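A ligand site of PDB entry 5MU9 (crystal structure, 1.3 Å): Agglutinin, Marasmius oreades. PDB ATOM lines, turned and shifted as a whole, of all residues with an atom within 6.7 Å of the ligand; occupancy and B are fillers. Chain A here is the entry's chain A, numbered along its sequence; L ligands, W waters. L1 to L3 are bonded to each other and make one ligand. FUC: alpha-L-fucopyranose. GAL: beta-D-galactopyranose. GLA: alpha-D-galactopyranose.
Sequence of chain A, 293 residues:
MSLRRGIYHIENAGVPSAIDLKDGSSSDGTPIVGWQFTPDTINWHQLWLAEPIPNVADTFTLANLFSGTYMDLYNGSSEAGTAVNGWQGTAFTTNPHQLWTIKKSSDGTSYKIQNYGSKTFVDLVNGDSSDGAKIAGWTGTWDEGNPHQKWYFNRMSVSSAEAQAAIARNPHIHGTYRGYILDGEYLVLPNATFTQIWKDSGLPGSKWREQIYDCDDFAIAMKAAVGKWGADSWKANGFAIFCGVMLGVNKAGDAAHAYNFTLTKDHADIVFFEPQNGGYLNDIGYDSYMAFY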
ATOM      1  N   HIS A   9      14.768   3.532  19.107  1.00  0.00           N
ATOM      2  CA  HIS A   9      13.358   3.324  18.883  1.00  0.00           C
ATOM      3  C   HIS A   9      13.292   2.457  17.618  1.00  0.00           C
ATOM      4  O   HIS A   9      13.848   2.877  16.595  1.00  0.00           O
ATOM      5  CB  HIS A   9      12.716   4.712  18.688  1.00  0.00           C
ATOM      6  CG  HIS A   9      11.241   4.636  18.589  1.00  0.00           C
ATOM      7  ND1 HIS A   9      10.527   4.818  17.420  1.00  0.00           N
ATOM      8  CD2 HIS A   9      10.354   4.363  19.565  1.00  0.00           C
ATOM      9  CE1 HIS A   9       9.269   4.630  17.687  1.00  0.00           C
ATOM     10  NE2 HIS A   9       9.138   4.435  18.991  1.00  0.00           N
ATOM     11  N   ASP A  20       7.396  -2.607  21.262  1.00  0.00           N
ATOM     12  CA  ASP A  20       6.869  -2.036  22.486  1.00  0.00           C
ATOM     13  C   ASP A  20       6.811  -3.146  23.530  1.00  0.00           C
ATOM     14  O   ASP A  20       6.193  -4.216  23.316  1.00  0.00           O
ATOM     15  CB  ASP A  20       5.491  -1.458  22.172  1.00  0.00           C
ATOM     16  CG  ASP A  20       4.789  -0.758  23.378  1.00  0.00           C
ATOM     17  OD1 ASP A  20       4.510  -1.471  24.353  1.00  0.00           O
ATOM     18  OD2 ASP A  20       4.456   0.442  23.236  1.00  0.00           O
ATOM     19  N   LEU A  21       7.379  -2.916  24.713  1.00  0.00           N
ATOM     20  CA  LEU A  21       7.218  -3.875  25.817  1.00  0.00           C
ATOM     21  C   LEU A  21       5.922  -3.535  26.521  1.00  0.00           C
ATOM     22  O   LEU A  21       5.734  -2.410  27.081  1.00  0.00           O
ATOM     23  CB  LEU A  21       8.397  -3.725  26.797  1.00  0.00           C
ATOM     24  CG  LEU A  21       8.267  -4.633  27.980  1.00  0.00           C
ATOM     25  CD1 LEU A  21       8.329  -6.140  27.663  1.00  0.00           C
ATOM     26  CD2 LEU A  21       9.413  -4.343  28.973  1.00  0.00           C
ATOM     27  N   LYS A  22       4.943  -4.419  26.435  1.00  0.00           N
ATOM     28  CA  LYS A  22       3.552  -4.098  26.779  1.00  0.00           C
ATOM     29  C   LYS A  22       3.429  -3.582  28.224  1.00  0.00           C
ATOM     30  O   LYS A  22       3.802  -4.251  29.167  1.00  0.00           O
ATOM     31  CB  LYS A  22       2.635  -5.293  26.516  1.00  0.00           C
ATOM     32  CG  LYS A  22       1.228  -4.837  26.339  1.00  0.00           C
ATOM     33  CD  LYS A  22       0.279  -6.007  25.896  1.00  0.00           C
ATOM     34  CE  LYS A  22      -1.123  -5.475  25.736  1.00  0.00           C
ATOM     35  NZ  LYS A  22      -2.054  -6.538  25.193  1.00  0.00           N
ATOM     36  N   ASP A  23       2.828  -2.394  28.310  1.00  0.00           N
ATOM     37  CA  ASP A  23       2.646  -1.677  29.590  1.00  0.00           C
ATOM     38  C   ASP A  23       3.945  -1.348  30.304  1.00  0.00           C
ATOM     39  O   ASP A  23       3.907  -0.993  31.521  1.00  0.00           O
ATOM     40  CB  ASP A  23       1.663  -2.421  30.529  1.00  0.00           C
ATOM     41  CG  ASP A  23       0.940  -1.501  31.519  1.00  0.00           C
ATOM     42  OD1 ASP A  23       0.611  -0.381  31.116  1.00  0.00           O
ATOM     43  OD2 ASP A  23       0.709  -1.928  32.698  1.00  0.00           O
ATOM     44  N   GLY A  24       5.074  -1.499  29.618  1.00  0.00           N
ATOM     45  CA  GLY A  24       6.356  -1.318  30.285  1.00  0.00           C
ATOM     46  C   GLY A  24       6.639  -2.309  31.411  1.00  0.00           C
ATOM     47  O   GLY A  24       7.489  -2.029  32.233  1.00  0.00           O
ATOM     48  N   VAL A  33       5.311  -6.311  21.619  1.00  0.00           N
ATOM     49  CA  VAL A  33       4.220  -6.104  20.618  1.00  0.00           C
ATOM     50  C   VAL A  33       4.505  -4.943  19.718  1.00  0.00           C
ATOM     51  O   VAL A  33       5.269  -4.016  20.066  1.00  0.00           O
ATOM     52  CB  VAL A  33       2.846  -5.977  21.287  1.00  0.00           C
ATOM     53  CG1 VAL A  33       2.461  -7.250  22.084  1.00  0.00           C
ATOM     54  CG2 VAL A  33       2.818  -4.737  22.214  1.00  0.00           C
ATOM     55  N   TRP A  35       3.232  -1.375  18.267  1.00  0.00           N
ATOM     56  CA  TRP A  35       2.338  -0.294  18.823  1.00  0.00           C
ATOM     57  C   TRP A  35       2.684   1.006  18.113  1.00  0.00           C
ATOM     58  O   TRP A  35       3.851   1.305  17.850  1.00  0.00           O
ATOM     59  CB  TRP A  35       2.577  -0.192  20.357  1.00  0.00           C
ATOM     60  CG  TRP A  35       1.423   0.392  21.139  1.00  0.00           C
ATOM     61  CD1 TRP A  35       0.974   1.691  21.211  1.00  0.00           C
ATOM     62  CD2 TRP A  35       0.506  -0.384  21.886  1.00  0.00           C
ATOM     63  NE1 TRP A  35      -0.192   1.788  21.977  1.00  0.00           N
ATOM     64  CE2 TRP A  35      -0.486   0.522  22.406  1.00  0.00           C
ATOM     65  CE3 TRP A  35       0.396  -1.733  22.197  1.00  0.00           C
ATOM     66  CZ2 TRP A  35      -1.538   0.042  23.210  1.00  0.00           C
ATOM     67  CZ3 TRP A  35      -0.650  -2.172  22.917  1.00  0.00           C
ATOM     68  CH2 TRP A  35      -1.555  -1.305  23.457  1.00  0.00           C
ATOM     69  N   GLN A  36       1.678   1.824  17.901  1.00  0.00           N
ATOM     70  CA  GLN A  36       1.906   3.169  17.290  1.00  0.00           C
ATOM     71  C   GLN A  36       2.675   4.026  18.228  1.00  0.00           C
ATOM     72  O   GLN A  36       2.782   3.814  19.476  1.00  0.00           O
ATOM     73  CB  GLN A  36       0.590   3.760  16.882  1.00  0.00           C
ATOM     74  CG  GLN A  36      -0.344   4.236  18.039  1.00  0.00           C
ATOM     75  CD  GLN A  36      -1.591   4.823  17.543  1.00  0.00           C
ATOM     76  OE1 GLN A  36      -1.566   5.854  16.882  1.00  0.00           O
ATOM     77  NE2 GLN A  36      -2.684   4.127  17.792  1.00  0.00           N
ATOM     78  N   PHE A  37       3.249   5.108  17.669  1.00  0.00           N
ATOM     79  CA  PHE A  37       4.125   5.989  18.428  1.00  0.00           C
ATOM     80  C   PHE A  37       3.918   7.419  18.028  1.00  0.00           C
ATOM     81  O   PHE A  37       3.235   7.723  17.010  1.00  0.00           O
ATOM     82  CB  PHE A  37       5.580   5.573  18.191  1.00  0.00           C
ATOM     83  CG  PHE A  37       6.067   5.706  16.794  1.00  0.00           C
ATOM     84  CD1 PHE A  37       5.986   4.668  15.891  1.00  0.00           C
ATOM     85  CD2 PHE A  37       6.707   6.870  16.393  1.00  0.00           C
ATOM     86  CE1 PHE A  37       6.465   4.773  14.644  1.00  0.00           C
ATOM     87  CE2 PHE A  37       7.182   6.959  15.109  1.00  0.00           C
ATOM     88  CZ  PHE A  37       7.052   5.908  14.282  1.00  0.00           C
ATOM     89  N   THR A  38       4.500   8.348  18.837  1.00  0.00           N
ATOM     90  CA  THR A  38       4.359   9.777  18.518  1.00  0.00           C
ATOM     91  C   THR A  38       5.784  10.273  18.295  1.00  0.00           C
ATOM     92  O   THR A  38       6.639  10.212  19.234  1.00  0.00           O
ATOM     93  CB  THR A  38       3.653  10.549  19.676  1.00  0.00           C
ATOM     94  OG1 THR A  38       2.404   9.914  19.982  1.00  0.00           O
ATOM     95  CG2 THR A  38       3.491  11.972  19.272  1.00  0.00           C
ATOM     96  N   PRO A  39       6.132  10.812  17.141  1.00  0.00           N
ATOM     97  CA  PRO A  39       7.473  11.324  16.897  1.00  0.00           C
ATOM     98  C   PRO A  39       7.773  12.502  17.791  1.00  0.00           C
ATOM     99  O   PRO A  39       6.860  13.178  18.218  1.00  0.00           O
ATOM    100  CB  PRO A  39       7.485  11.802  15.435  1.00  0.00           C
ATOM    101  CG  PRO A  39       6.325  11.006  14.847  1.00  0.00           C
ATOM    102  CD  PRO A  39       5.285  10.932  15.915  1.00  0.00           C
ATOM    103  N   THR A  41       8.676  12.688  20.847  1.00  0.00           N
ATOM    104  CA  THR A  41       8.329  12.406  22.276  1.00  0.00           C
ATOM    105  C   THR A  41       9.283  11.359  22.823  1.00  0.00           C
ATOM    106  O   THR A  41       9.943  10.607  22.084  1.00  0.00           O
ATOM    107  CB  THR A  41       6.883  11.932  22.423  1.00  0.00           C
ATOM    108  OG1 THR A  41       6.747  10.576  21.988  1.00  0.00           O
ATOM    109  CG2 THR A  41       5.862  12.866  21.794  1.00  0.00           C
ATOM    110  N   ILE A  42       9.298  11.224  24.166  1.00  0.00           N
ATOM    111  CA  ILE A  42       9.698  10.002  24.773  1.00  0.00           C
ATOM    112  C   ILE A  42       8.574   8.994  24.692  1.00  0.00           C
ATOM    113  O   ILE A  42       7.479   9.157  25.249  1.00  0.00           O
ATOM    114  CB  ILE A  42      10.136  10.245  26.258  1.00  0.00           C
ATOM    115  CG1 ILE A  42      11.382  11.182  26.325  1.00  0.00           C
ATOM    116  CG2 ILE A  42      10.379   8.918  26.939  1.00  0.00           C
ATOM    117  CD1 ILE A  42      12.650  10.708  25.690  1.00  0.00           C
ATOM    118  N   ASN A  43       8.852   7.911  23.927  1.00  0.00           N
ATOM    119  CA  ASN A  43       7.888   6.805  23.806  1.00  0.00           C
ATOM    120  C   ASN A  43       8.326   5.813  24.855  1.00  0.00           C
ATOM    121  O   ASN A  43       9.244   4.979  24.679  1.00  0.00           O
ATOM    122  CB  ASN A  43       7.914   6.210  22.408  1.00  0.00           C
ATOM    123  CG  ASN A  43       7.283   7.120  21.375  1.00  0.00           C
ATOM    124  OD1 ASN A  43       6.073   7.210  21.319  1.00  0.00           O
ATOM    125  ND2 ASN A  43       8.092   7.785  20.599  1.00  0.00           N
ATOM    126  N   TRP A  44       7.685   5.925  26.032  1.00  0.00           N
ATOM    127  CA  TRP A  44       8.123   5.347  27.285  1.00  0.00           C
ATOM    128  C   TRP A  44       8.376   3.816  27.321  1.00  0.00           C
ATOM    129  O   TRP A  44       9.257   3.360  28.047  1.00  0.00           O
ATOM    130  CB  TRP A  44       7.127   5.706  28.433  1.00  0.00           C
ATOM    131  CG  TRP A  44       7.319   7.095  28.900  1.00  0.00           C
ATOM    132  CD1 TRP A  44       6.647   8.173  28.507  1.00  0.00           C
ATOM    133  CD2 TRP A  44       8.298   7.549  29.840  1.00  0.00           C
ATOM    134  NE1 TRP A  44       7.091   9.282  29.146  1.00  0.00           N
ATOM    135  CE2 TRP A  44       8.146   8.943  29.942  1.00  0.00           C
ATOM    136  CE3 TRP A  44       9.260   6.919  30.562  1.00  0.00           C
ATOM    137  CZ2 TRP A  44       8.917   9.696  30.777  1.00  0.00           C
ATOM    138  CZ3 TRP A  44      10.037   7.636  31.353  1.00  0.00           C
ATOM    139  CH2 TRP A  44       9.902   9.012  31.481  1.00  0.00           C
ATOM    140  N   HIS A  45       7.601   3.018  26.525  1.00  0.00           N
ATOM    141  CA  HIS A  45       7.720   1.612  26.551  1.00  0.00           C
ATOM    142  C   HIS A  45       8.500   1.055  25.310  1.00  0.00           C
ATOM    143  O   HIS A  45       8.565  -0.180  25.148  1.00  0.00           O
ATOM    144  CB  HIS A  45       6.349   0.935  26.653  1.00  0.00           C
ATOM    145  CG  HIS A  45       5.597   1.412  27.829  1.00  0.00           C
ATOM    146  ND1 HIS A  45       4.229   1.315  27.902  1.00  0.00           N
ATOM    147  CD2 HIS A  45       5.979   1.944  29.016  1.00  0.00           C
ATOM    148  CE1 HIS A  45       3.794   1.775  29.061  1.00  0.00           C
ATOM    149  NE2 HIS A  45       4.847   2.175  29.770  1.00  0.00           N
ATOM    150  N   GLN A  46       9.082   1.986  24.513  1.00  0.00           N
ATOM    151  CA  GLN A  46       9.564   1.646  23.163  1.00  0.00           C
ATOM    152  C   GLN A  46      11.038   2.006  22.979  1.00  0.00           C
ATOM    153  O   GLN A  46      11.457   2.195  21.846  1.00  0.00           O
ATOM    154  CB  GLN A  46       8.693   2.368  22.124  1.00  0.00           C
ATOM    155  CG  GLN A  46       7.213   2.009  22.189  1.00  0.00           C
ATOM    156  CD  GLN A  46       6.330   2.756  21.203  1.00  0.00           C
ATOM    157  OE1 GLN A  46       6.805   3.680  20.504  1.00  0.00           O
ATOM    158  NE2 GLN A  46       5.021   2.460  21.223  1.00  0.00           N
ATOM    159  N   PHE A  66      12.885   1.392  30.026  1.00  0.00           N
ATOM    160  CA  PHE A  66      11.968   1.579  31.147  1.00  0.00           C
ATOM    161  C   PHE A  66      11.941   0.405  32.138  1.00  0.00           C
ATOM    162  O   PHE A  66      12.076   0.659  33.359  1.00  0.00           O
ATOM    163  CB  PHE A  66      10.569   1.883  30.600  1.00  0.00           C
ATOM    164  CG  PHE A  66       9.537   2.117  31.695  1.00  0.00           C
ATOM    165  CD1 PHE A  66       9.488   3.373  32.309  1.00  0.00           C
ATOM    166  CD2 PHE A  66       8.677   1.161  32.067  1.00  0.00           C
ATOM    167  CE1 PHE A  66       8.566   3.635  33.296  1.00  0.00           C
ATOM    168  CE2 PHE A  66       7.683   1.418  33.026  1.00  0.00           C
ATOM    169  CZ  PHE A  66       7.674   2.623  33.673  1.00  0.00           C
ATOM    170  N   ASP A 131      -2.477  -1.819  17.458  1.00  0.00           N
ATOM    171  CA  ASP A 131      -1.768  -1.687  18.718  1.00  0.00           C
ATOM    172  C   ASP A 131      -1.859  -2.995  19.469  1.00  0.00           C
ATOM    173  O   ASP A 131      -3.041  -3.482  19.765  1.00  0.00           O
ATOM    174  CB  ASP A 131      -2.314  -0.557  19.559  1.00  0.00           C
ATOM    175  CG  ASP A 131      -2.060   0.836  18.864  1.00  0.00           C
ATOM    176  OD1 ASP A 131      -1.092   0.966  18.158  1.00  0.00           O
ATOM    177  OD2 ASP A 131      -2.824   1.807  19.253  1.00  0.00           O
HETATM  178  C1  FUC L   1       1.515   6.211  26.721  1.00  0.00           C
HETATM  179  C2  FUC L   1       0.555   7.346  27.023  1.00  0.00           C
HETATM  180  C3  FUC L   1       0.153   7.289  28.477  1.00  0.00           C
HETATM  181  C4  FUC L   1       1.336   7.292  29.387  1.00  0.00           C
HETATM  182  C5  FUC L   1       2.224   6.082  28.987  1.00  0.00           C
HETATM  183  C6  FUC L   1       3.450   5.943  29.834  1.00  0.00           C
HETATM  184  O2  FUC L   1      -0.634   7.211  26.159  1.00  0.00           O
HETATM  185  O3  FUC L   1      -0.732   8.462  28.739  1.00  0.00           O
HETATM  186  O4  FUC L   1       2.058   8.511  29.334  1.00  0.00           O
HETATM  187  O5  FUC L   1       2.629   6.221  27.633  1.00  0.00           O
HETATM  188  C1  GAL L   2       0.763   2.770  27.222  1.00  0.00           C
HETATM  189  C2  GAL L   2       1.563   3.827  26.472  1.00  0.00           C
HETATM  190  C3  GAL L   2       1.588   3.503  25.004  1.00  0.00           C
HETATM  191  C4  GAL L   2       2.064   2.107  24.731  1.00  0.00           C
HETATM  192  C5  GAL L   2       1.225   1.109  25.561  1.00  0.00           C
HETATM  193  C6  GAL L   2       1.641  -0.350  25.431  1.00  0.00           C
HETATM  194  O1  GAL L   2       0.931   2.966  28.591  1.00  0.00           O
HETATM  195  O2  GAL L   2       0.797   5.026  26.707  1.00  0.00           O
HETATM  196  O3  GAL L   2       2.345   4.540  24.405  1.00  0.00           O
HETATM  197  O4  GAL L   2       3.450   1.986  25.042  1.00  0.00           O
HETATM  198  O5  GAL L   2       1.322   1.486  26.975  1.00  0.00           O
HETATM  199  O6  GAL L   2       2.868  -0.612  26.125  1.00  0.00           O
HETATM  200  C1  GLA L   3       2.471   4.456  22.960  1.00  0.00           C
HETATM  201  C2  GLA L   3       3.249   5.646  22.416  1.00  0.00           C
HETATM  202  C3  GLA L   3       2.449   6.937  22.471  1.00  0.00           C
HETATM  203  C4  GLA L   3       1.094   6.777  21.848  1.00  0.00           C
HETATM  204  C5  GLA L   3       0.410   5.612  22.581  1.00  0.00           C
HETATM  205  C6  GLA L   3      -0.988   5.292  22.096  1.00  0.00           C
HETATM  206  O2  GLA L   3       4.493   5.829  23.098  1.00  0.00           O
HETATM  207  O3  GLA L   3       3.128   8.008  21.802  1.00  0.00           O
HETATM  208  O4  GLA L   3       1.210   6.471  20.429  1.00  0.00           O
HETATM  209  O5  GLA L   3       1.180   4.431  22.359  1.00  0.00           O
HETATM  210  O6  GLA L   3      -1.595   4.217  22.834  1.00  0.00           O
HETATM  211  O   HOH W   1      -3.598   2.685  21.759  1.00  0.00           O
HETATM  212  O   HOH W   2      -0.654   8.940  31.590  1.00  0.00           O
HETATM  213  O   HOH W   3       4.971   7.327  25.666  1.00  0.00           O
HETATM  214  O   HOH W   4       4.855   9.231  23.518  1.00  0.00           O
HETATM  215  O   HOH W   5       5.485   3.851  24.831  1.00  0.00           O
HETATM  216  O   HOH W   6      -2.076   4.864  25.543  1.00  0.00           O
HETATM  217  O   HOH W   7       3.456   9.228  27.041  1.00  0.00           O
HETATM  218  O   HOH W   8      -0.376  -0.187  28.547  1.00  0.00           O
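An oxygen (O6) of GAL L2 sits at hydrogen-bond distance from the side-chain carboxylate (OD1) of Asp 20. The backbone NH (N) of Thr 38 lies within hydrogen-bond range of an oxygen (O3) of GLA L3. An oxygen (O3) of GLA L3 lies within hydrogen-bond range of the side-chain hydroxyl of Thr 38, at 2.7 Å. O2 of GLA L3 is in hydrogen-bond range of OD1 of Asn 43 (2.8 Å). The backbone NH (N) of Asp 23 is in hydrogen-bond range of an oxygen (O6) of GAL L2 (2.8 Å). NE1 of Trp 35 is in hydrogen-bond range of O6 of GLA L3 (2.9 Å). An oxygen (O6) of GAL L2 lies within hydrogen-bond range of a ring nitrogen (ND1) of His 45. An oxygen (O4) of GLA L3 sits at hydrogen-bond distance from the backbone carbonyl oxygen of Gln 36 (3.2 Å).
The side-chain carboxylate (OD2) of Asp 20 is in hydrogen-bond range of the side-chain amide nitrogen (NE2) of Gln 46 (2.9 Å). N of Asp 20 sits at hydrogen-bond distance from O of Val 33, 2.8 Å away. ND2 of Asn 43 lies within hydrogen-bond range of O of Thr 38, 3.1 Å away. OG1 of Thr 41 sits at hydrogen-bond distance from O of Thr 38, 2.8 Å away. The side-chain amide nitrogen (ND2) of Asn 43 sits at hydrogen-bond distance from the side-chain hydroxyl (OG1) of Thr 41, at 3.4 Å. O of His 45 is in hydrogen-bond range of N of Leu 21 (3.0 Å). The backbone carbonyl oxygen (O) of Gln 36 lies within hydrogen-bond range of the side-chain amide nitrogen (NE2) of Gln 46, at 3.1 Å. OE1 of Gln 46 lies within hydrogen-bond range of NE2 of His 9 (2.9 Å).
O of Leu 21 touches O6 of GAL L2, 3.5 Å away. Lys 22 touches the ligand. CA of Phe 37 touches O4 of GLA L3, 3.6 Å away. CB of Trp 44 touches C6 of FUC L1, at 3.9 Å. NE2 of Gln 46 touches C1 of GLA L3, 3.7 Å away. Along chain A the residues within 4 Å of the ligand span positions 20 to 46. The nearest printed residue that does not touch the ligand is Gly 24 (4.2 Å).
Water W4 lies within hydrogen-bond range of an oxygen (O3) of GLA L3, the side-chain hydroxyl (OG1) of Thr 41, the backbone carbonyl oxygen (O) of Ile 42 and the side-chain amide oxygen (OD1) of Asn 43. Water W1 bridges an oxygen (O6) of GLA L3 and the side-chain carboxylate (OD2) of Asp 131. Water W5 lies within hydrogen-bond range of O4 of GAL L2 (2.8 Å), N of His 45 (2.8 Å) and N of Trp 44 (3.3 Å). Water W8 bridges OD1 of Asp 23 (2.8 Å) and O5 of GAL L2 (2.9 Å). Water W3 lies within hydrogen-bond range of an oxygen (O2) of GLA L3 (3.0 Å), the backbone NH (N) of Trp 44 (3.1 Å) and the backbone carbonyl oxygen (O) of Ile 42 (3.1 Å).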
